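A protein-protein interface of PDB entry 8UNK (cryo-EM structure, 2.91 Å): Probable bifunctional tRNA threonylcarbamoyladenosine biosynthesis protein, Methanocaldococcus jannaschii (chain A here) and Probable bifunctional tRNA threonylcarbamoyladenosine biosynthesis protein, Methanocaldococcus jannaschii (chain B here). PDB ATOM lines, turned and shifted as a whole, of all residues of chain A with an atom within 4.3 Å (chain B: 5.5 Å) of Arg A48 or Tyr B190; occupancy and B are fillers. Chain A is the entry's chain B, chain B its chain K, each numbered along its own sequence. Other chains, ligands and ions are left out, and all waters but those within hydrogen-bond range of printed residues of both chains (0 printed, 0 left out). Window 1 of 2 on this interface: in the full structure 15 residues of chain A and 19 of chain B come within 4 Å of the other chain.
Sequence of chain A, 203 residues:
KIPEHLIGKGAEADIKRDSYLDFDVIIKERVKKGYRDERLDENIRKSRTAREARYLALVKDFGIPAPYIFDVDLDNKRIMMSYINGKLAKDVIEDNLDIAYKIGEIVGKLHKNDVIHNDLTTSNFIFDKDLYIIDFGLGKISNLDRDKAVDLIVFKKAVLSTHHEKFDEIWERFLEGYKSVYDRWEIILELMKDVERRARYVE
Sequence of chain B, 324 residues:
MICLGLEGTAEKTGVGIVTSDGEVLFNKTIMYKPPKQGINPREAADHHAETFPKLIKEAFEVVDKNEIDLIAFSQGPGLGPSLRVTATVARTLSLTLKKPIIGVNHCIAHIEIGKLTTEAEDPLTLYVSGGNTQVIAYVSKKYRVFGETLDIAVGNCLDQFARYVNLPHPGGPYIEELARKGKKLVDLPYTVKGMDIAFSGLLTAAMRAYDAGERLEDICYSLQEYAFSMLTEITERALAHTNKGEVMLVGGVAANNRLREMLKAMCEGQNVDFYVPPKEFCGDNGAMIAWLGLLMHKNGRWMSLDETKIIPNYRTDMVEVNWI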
ATOM      1  N   ARG A  30      -5.202   3.583  10.882  1.00  0.00           N
ATOM      2  CA  ARG A  30      -5.990   2.427  10.453  1.00  0.00           C
ATOM      3  C   ARG A  30      -5.598   2.102   9.014  1.00  0.00           C
ATOM      4  O   ARG A  30      -6.232   2.530   8.049  1.00  0.00           O
ATOM      5  CB  ARG A  30      -7.484   2.707  10.584  1.00  0.00           C
ATOM      6  CG  ARG A  30      -7.864   3.563  11.778  1.00  0.00           C
ATOM      7  CD  ARG A  30      -7.415   2.944  13.091  1.00  0.00           C
ATOM      8  NE  ARG A  30      -8.250   1.817  13.487  1.00  0.00           N
ATOM      9  CZ  ARG A  30      -9.376   1.921  14.181  1.00  0.00           C
ATOM     10  NH1 ARG A  30      -9.847   3.095  14.570  1.00  0.00           N
ATOM     11  NH2 ARG A  30     -10.048   0.817  14.494  1.00  0.00           N
ATOM     12  N   ILE A  44     -14.841   1.770   6.551  1.00  0.00           N
ATOM     13  CA  ILE A  44     -14.740   1.242   7.905  1.00  0.00           C
ATOM     14  C   ILE A  44     -13.594   1.902   8.652  1.00  0.00           C
ATOM     15  O   ILE A  44     -13.703   2.177   9.849  1.00  0.00           O
ATOM     16  CB  ILE A  44     -14.595  -0.290   7.866  1.00  0.00           C
ATOM     17  CG1 ILE A  44     -15.982  -0.936   7.823  1.00  0.00           C
ATOM     18  CG2 ILE A  44     -13.790  -0.794   9.062  1.00  0.00           C
ATOM     19  CD1 ILE A  44     -15.960  -2.423   7.603  1.00  0.00           C
ATOM     20  N   ARG A  45     -12.474   2.162   7.975  1.00  0.00           N
ATOM     21  CA  ARG A  45     -11.379   2.852   8.646  1.00  0.00           C
ATOM     22  C   ARG A  45     -11.816   4.232   9.118  1.00  0.00           C
ATOM     23  O   ARG A  45     -11.536   4.625  10.257  1.00  0.00           O
ATOM     24  CB  ARG A  45     -10.172   2.965   7.716  1.00  0.00           C
ATOM     25  CG  ARG A  45      -9.571   1.635   7.315  1.00  0.00           C
ATOM     26  CD  ARG A  45      -8.922   1.717   5.948  1.00  0.00           C
ATOM     27  NE  ARG A  45      -7.935   2.789   5.874  1.00  0.00           N
ATOM     28  CZ  ARG A  45      -7.700   3.530   4.799  1.00  0.00           C
ATOM     29  NH1 ARG A  45      -8.357   3.341   3.667  1.00  0.00           N
ATOM     30  NH2 ARG A  45      -6.776   4.486   4.861  1.00  0.00           N
ATOM     31  N   LYS A  46     -12.518   4.978   8.261  1.00  0.00           N
ATOM     32  CA  LYS A  46     -12.988   6.303   8.647  1.00  0.00           C
ATOM     33  C   LYS A  46     -13.970   6.217   9.808  1.00  0.00           C
ATOM     34  O   LYS A  46     -13.871   6.977  10.780  1.00  0.00           O
ATOM     35  CB  LYS A  46     -13.639   6.996   7.451  1.00  0.00           C
ATOM     36  CG  LYS A  46     -13.870   8.483   7.653  1.00  0.00           C
ATOM     37  CD  LYS A  46     -14.411   9.140   6.393  1.00  0.00           C
ATOM     38  CE  LYS A  46     -15.596  10.044   6.696  1.00  0.00           C
ATOM     39  NZ  LYS A  46     -15.754  11.122   5.680  1.00  0.00           N
ATOM     40  N   SER A  47     -14.931   5.295   9.722  1.00  0.00           N
ATOM     41  CA  SER A  47     -15.927   5.176  10.781  1.00  0.00           C
ATOM     42  C   SER A  47     -15.277   4.799  12.104  1.00  0.00           C
ATOM     43  O   SER A  47     -15.639   5.335  13.157  1.00  0.00           O
ATOM     44  CB  SER A  47     -16.986   4.144  10.395  1.00  0.00           C
ATOM     45  OG  SER A  47     -18.068   4.757   9.719  1.00  0.00           O
ATOM     46  N   ARG A  48     -14.311   3.883  12.070  1.00  0.00           N
ATOM     47  CA  ARG A  48     -13.666   3.449  13.300  1.00  0.00           C
ATOM     48  C   ARG A  48     -12.794   4.551  13.881  1.00  0.00           C
ATOM     49  O   ARG A  48     -12.748   4.724  15.101  1.00  0.00           O
ATOM     50  CB  ARG A  48     -12.846   2.190  13.041  1.00  0.00           C
ATOM     51  CG  ARG A  48     -13.680   0.927  13.067  1.00  0.00           C
ATOM     52  CD  ARG A  48     -12.837  -0.305  12.842  1.00  0.00           C
ATOM     53  NE  ARG A  48     -13.623  -1.523  12.981  1.00  0.00           N
ATOM     54  CZ  ARG A  48     -13.177  -2.737  12.688  1.00  0.00           C
ATOM     55  NH1 ARG A  48     -11.950  -2.934  12.239  1.00  0.00           N
ATOM     56  NH2 ARG A  48     -13.983  -3.779  12.859  1.00  0.00           N
ATOM     57  N   THR A  49     -12.105   5.314  13.031  1.00  0.00           N
ATOM     58  CA  THR A  49     -11.334   6.445  13.536  1.00  0.00           C
ATOM     59  C   THR A  49     -12.244   7.476  14.192  1.00  0.00           C
ATOM     60  O   THR A  49     -11.946   7.978  15.284  1.00  0.00           O
ATOM     61  CB  THR A  49     -10.533   7.079  12.398  1.00  0.00           C
ATOM     62  OG1 THR A  49      -9.739   6.074  11.754  1.00  0.00           O
ATOM     63  CG2 THR A  49      -9.621   8.174  12.918  1.00  0.00           C
ATOM     64  N   ALA A  50     -13.373   7.789  13.551  1.00  0.00           N
ATOM     65  CA  ALA A  50     -14.298   8.766  14.116  1.00  0.00           C
ATOM     66  C   ALA A  50     -14.865   8.283  15.445  1.00  0.00           C
ATOM     67  O   ALA A  50     -14.913   9.037  16.425  1.00  0.00           O
ATOM     68  CB  ALA A  50     -15.425   9.051  13.125  1.00  0.00           C
ATOM     69  N   ARG A  51     -15.308   7.025  15.497  1.00  0.00           N
ATOM     70  CA  ARG A  51     -15.863   6.492  16.736  1.00  0.00           C
ATOM     71  C   ARG A  51     -14.813   6.452  17.836  1.00  0.00           C
ATOM     72  O   ARG A  51     -15.097   6.804  18.987  1.00  0.00           O
ATOM     73  CB  ARG A  51     -16.439   5.099  16.499  1.00  0.00           C
ATOM     74  CG  ARG A  51     -17.829   5.106  15.888  1.00  0.00           C
ATOM     75  CD  ARG A  51     -18.621   3.878  16.294  1.00  0.00           C
ATOM     76  NE  ARG A  51     -18.050   2.652  15.748  1.00  0.00           N
ATOM     77  CZ  ARG A  51     -18.345   2.150  14.557  1.00  0.00           C
ATOM     78  NH1 ARG A  51     -19.204   2.748  13.746  1.00  0.00           N
ATOM     79  NH2 ARG A  51     -17.764   1.019  14.169  1.00  0.00           N
ATOM     80  N   GLU A  52     -13.593   6.022  17.507  1.00  0.00           N
ATOM     81  CA  GLU A  52     -12.539   5.976  18.509  1.00  0.00           C
ATOM     82  C   GLU A  52     -12.266   7.363  19.064  1.00  0.00           C
ATOM     83  O   GLU A  52     -12.179   7.545  20.280  1.00  0.00           O
ATOM     84  CB  GLU A  52     -11.266   5.382  17.914  1.00  0.00           C
ATOM     85  CG  GLU A  52     -10.023   5.668  18.737  1.00  0.00           C
ATOM     86  CD  GLU A  52      -8.946   4.622  18.550  1.00  0.00           C
ATOM     87  OE1 GLU A  52      -9.166   3.462  18.955  1.00  0.00           O
ATOM     88  OE2 GLU A  52      -7.876   4.960  18.002  1.00  0.00           O
ATOM     89  N   GLY A 137     -12.260   1.607  19.466  1.00  0.00           N
ATOM     90  CA  GLY A 137     -12.650   1.652  18.065  1.00  0.00           C
ATOM     91  C   GLY A 137     -14.096   1.263  17.828  1.00  0.00           C
ATOM     92  O   GLY A 137     -14.799   1.907  17.046  1.00  0.00           O
ATOM     93  N   LEU A 138     -14.561   0.209  18.494  1.00  0.00           N
ATOM     94  CA  LEU A 138     -15.882  -0.350  18.241  1.00  0.00           C
ATOM     95  C   LEU A 138     -16.931   0.130  19.235  1.00  0.00           C
ATOM     96  O   LEU A 138     -18.056  -0.379  19.221  1.00  0.00           O
ATOM     97  CB  LEU A 138     -15.811  -1.876  18.251  1.00  0.00           C
ATOM     98  CG  LEU A 138     -15.184  -2.497  17.003  1.00  0.00           C
ATOM     99  CD1 LEU A 138     -13.800  -3.041  17.313  1.00  0.00           C
ATOM    100  CD2 LEU A 138     -16.080  -3.585  16.441  1.00  0.00           C
ATOM    101  N   LEU B 188     -23.923  -2.016   5.839  1.00  0.00           N
ATOM    102  CA  LEU B 188     -24.432  -2.948   6.831  1.00  0.00           C
ATOM    103  C   LEU B 188     -23.458  -2.989   7.997  1.00  0.00           C
ATOM    104  O   LEU B 188     -22.266  -2.707   7.822  1.00  0.00           O
ATOM    105  CB  LEU B 188     -24.612  -4.360   6.251  1.00  0.00           C
ATOM    106  CG  LEU B 188     -25.127  -4.460   4.813  1.00  0.00           C
ATOM    107  CD1 LEU B 188     -24.800  -5.818   4.219  1.00  0.00           C
ATOM    108  CD2 LEU B 188     -26.625  -4.205   4.766  1.00  0.00           C
ATOM    109  N   PRO B 189     -23.927  -3.335   9.193  1.00  0.00           N
ATOM    110  CA  PRO B 189     -23.042  -3.303  10.358  1.00  0.00           C
ATOM    111  C   PRO B 189     -21.918  -4.312  10.231  1.00  0.00           C
ATOM    112  O   PRO B 189     -22.088  -5.407   9.695  1.00  0.00           O
ATOM    113  CB  PRO B 189     -23.973  -3.645  11.526  1.00  0.00           C
ATOM    114  CG  PRO B 189     -25.072  -4.422  10.922  1.00  0.00           C
ATOM    115  CD  PRO B 189     -25.215  -3.980   9.496  1.00  0.00           C
ATOM    116  N   TYR B 190     -20.756  -3.925  10.743  1.00  0.00           N
ATOM    117  CA  TYR B 190     -19.556  -4.755  10.749  1.00  0.00           C
ATOM    118  C   TYR B 190     -19.243  -5.048  12.212  1.00  0.00           C
ATOM    119  O   TYR B 190     -18.457  -4.345  12.848  1.00  0.00           O
ATOM    120  CB  TYR B 190     -18.420  -4.030  10.037  1.00  0.00           C
ATOM    121  CG  TYR B 190     -17.137  -4.814   9.881  1.00  0.00           C
ATOM    122  CD1 TYR B 190     -16.264  -4.979  10.944  1.00  0.00           C
ATOM    123  CD2 TYR B 190     -16.782  -5.360   8.658  1.00  0.00           C
ATOM    124  CE1 TYR B 190     -15.090  -5.681  10.797  1.00  0.00           C
ATOM    125  CE2 TYR B 190     -15.608  -6.060   8.503  1.00  0.00           C
ATOM    126  CZ  TYR B 190     -14.765  -6.217   9.578  1.00  0.00           C
ATOM    127  OH  TYR B 190     -13.590  -6.914   9.439  1.00  0.00           O
ATOM    128  N   THR B 191     -19.874  -6.092  12.747  1.00  0.00           N
ATOM    129  CA  THR B 191     -19.788  -6.416  14.166  1.00  0.00           C
ATOM    130  C   THR B 191     -18.623  -7.371  14.392  1.00  0.00           C
ATOM    131  O   THR B 191     -18.672  -8.528  13.965  1.00  0.00           O
ATOM    132  CB  THR B 191     -21.093  -7.034  14.657  1.00  0.00           C
ATOM    133  OG1 THR B 191     -21.499  -8.071  13.756  1.00  0.00           O
ATOM    134  CG2 THR B 191     -22.186  -5.982  14.737  1.00  0.00           C
ATOM    135  N   VAL B 192     -17.580  -6.891  15.062  1.00  0.00           N
ATOM    136  CA  VAL B 192     -16.456  -7.737  15.445  1.00  0.00           C
ATOM    137  C   VAL B 192     -16.096  -7.446  16.894  1.00  0.00           C
ATOM    138  O   VAL B 192     -15.372  -6.489  17.185  1.00  0.00           O
ATOM    139  CB  VAL B 192     -15.248  -7.519  14.522  1.00  0.00           C
ATOM    140  CG1 VAL B 192     -14.056  -8.333  15.007  1.00  0.00           C
ATOM    141  CG2 VAL B 192     -15.609  -7.890  13.104  1.00  0.00           C
ATOM    142  N   LEU B 202     -25.684  -8.866  10.712  1.00  0.00           N
ATOM    143  CA  LEU B 202     -25.469  -8.805   9.271  1.00  0.00           C
ATOM    144  C   LEU B 202     -26.667  -9.339   8.507  1.00  0.00           C
ATOM    145  O   LEU B 202     -27.087  -8.749   7.508  1.00  0.00           O
ATOM    146  CB  LEU B 202     -24.224  -9.599   8.893  1.00  0.00           C
ATOM    147  CG  LEU B 202     -22.901  -8.881   9.102  1.00  0.00           C
ATOM    148  CD1 LEU B 202     -22.684  -7.920   7.942  1.00  0.00           C
ATOM    149  CD2 LEU B 202     -22.859  -8.156  10.442  1.00  0.00           C
ATOM    150  N   TYR B 226     -18.657  -8.218   3.687  1.00  0.00           N
ATOM    151  CA  TYR B 226     -18.721  -8.013   5.128  1.00  0.00           C
ATOM    152  C   TYR B 226     -18.319  -9.276   5.877  1.00  0.00           C
ATOM    153  O   TYR B 226     -17.370  -9.267   6.672  1.00  0.00           O
ATOM    154  CB  TYR B 226     -20.136  -7.593   5.535  1.00  0.00           C
ATOM    155  CG  TYR B 226     -20.441  -6.123   5.357  1.00  0.00           C
ATOM    156  CD1 TYR B 226     -19.685  -5.153   5.998  1.00  0.00           C
ATOM    157  CD2 TYR B 226     -21.503  -5.708   4.566  1.00  0.00           C
ATOM    158  CE1 TYR B 226     -19.966  -3.812   5.841  1.00  0.00           C
ATOM    159  CE2 TYR B 226     -21.790  -4.369   4.404  1.00  0.00           C
ATOM    160  CZ  TYR B 226     -21.019  -3.425   5.044  1.00  0.00           C
ATOM    161  OH  TYR B 226     -21.305  -2.089   4.886  1.00  0.00           O
ATOM    162  N   SER B 229     -14.853 -10.588   5.387  1.00  0.00           N
ATOM    163  CA  SER B 229     -13.893  -9.647   5.946  1.00  0.00           C
ATOM    164  C   SER B 229     -13.776  -9.810   7.455  1.00  0.00           C
ATOM    165  O   SER B 229     -12.669  -9.778   7.999  1.00  0.00           O
ATOM    166  CB  SER B 229     -14.303  -8.223   5.582  1.00  0.00           C
ATOM    167  OG  SER B 229     -15.712  -8.085   5.621  1.00  0.00           O
ATOM    168  N   MET B 230     -14.900  -9.989   8.151  1.00  0.00           N
ATOM    169  CA  MET B 230     -14.808 -10.211   9.594  1.00  0.00           C
ATOM    170  C   MET B 230     -14.156 -11.549   9.901  1.00  0.00           C
ATOM    171  O   MET B 230     -13.367 -11.659  10.846  1.00  0.00           O
ATOM    172  CB  MET B 230     -16.172 -10.136  10.276  1.00  0.00           C
ATOM    173  CG  MET B 230     -17.201  -9.361   9.542  1.00  0.00           C
ATOM    174  SD  MET B 230     -18.766  -9.240  10.391  1.00  0.00           S
ATOM    175  CE  MET B 230     -19.736  -8.788   8.977  1.00  0.00           C
ATOM    176  N   GLU B 233     -10.563 -11.012   9.489  1.00  0.00           N
ATOM    177  CA  GLU B 233      -9.968 -10.206  10.547  1.00  0.00           C
ATOM    178  C   GLU B 233      -9.796 -11.012  11.828  1.00  0.00           C
ATOM    179  O   GLU B 233      -8.766 -10.901  12.500  1.00  0.00           O
ATOM    180  CB  GLU B 233     -10.818  -8.963  10.802  1.00  0.00           C
ATOM    181  CG  GLU B 233     -10.004  -7.754  11.233  1.00  0.00           C
ATOM    182  CD  GLU B 233     -10.749  -6.861  12.200  1.00  0.00           C
ATOM    183  OE1 GLU B 233     -10.121  -6.375  13.165  1.00  0.00           O
ATOM    184  OE2 GLU B 233     -11.960  -6.641  11.992  1.00  0.00           O
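The guanidinium group (NH1) of Arg A30 sits close to the backbone carbonyl oxygen (O) of Arg A48 (3.4 Å). The side-chain carboxylate (OE2) of Glu B233 lies within hydrogen-bond range of the side-chain hydroxyl (OH) of Tyr B190, at 3.0 Å. The side-chain hydroxyl (OH) of Tyr B190 is in hydrogen-bond range of the backbone carbonyl oxygen (O) of Ser B229 (3.3 Å).
Of chain B, only Tyr B190 and Glu B233 come within 4 Å of Arg A48. Printed residues of chain A within 4 Å of Val B192: Leu A138 (3.1 Å). Printed residues of chain A within 4 Å of Glu B233: Arg A48. Printed residues of chain B within 4 Å of Ile A44: Tyr B190. The nearest printed residue of chain A that does not touch Val B192 is Arg A48 (4.3 Å).
The guanidinium group (NH2) of Arg A48 lies within salt-bridge range of the side-chain carboxylate (OE2) of Glu B233 (3.6 Å).
Ile A44 touches Tyr B190 (CD1 to CD2, 3.2 Å). NH2 of Arg A48 touches CE1 of Tyr B190, 3.0 Å away. CD2 of Leu A138 touches O of Val B192 (3.1 Å).
Printed residues of chain A that touch a printed residue of chain B: Ile A44, Arg A48 and Leu A138. Hydrophobic or aromatic side chains of chain B that line the printed part of chain A: Tyr B190. Among the printed residues, 4 pairs touch across the chains. Among the printed residues, Asp or Glu carboxylates within 4 Å of a Lys or Arg side-chain nitrogen of the other chain: Arg A48 with Glu B233 (3.6 Å).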
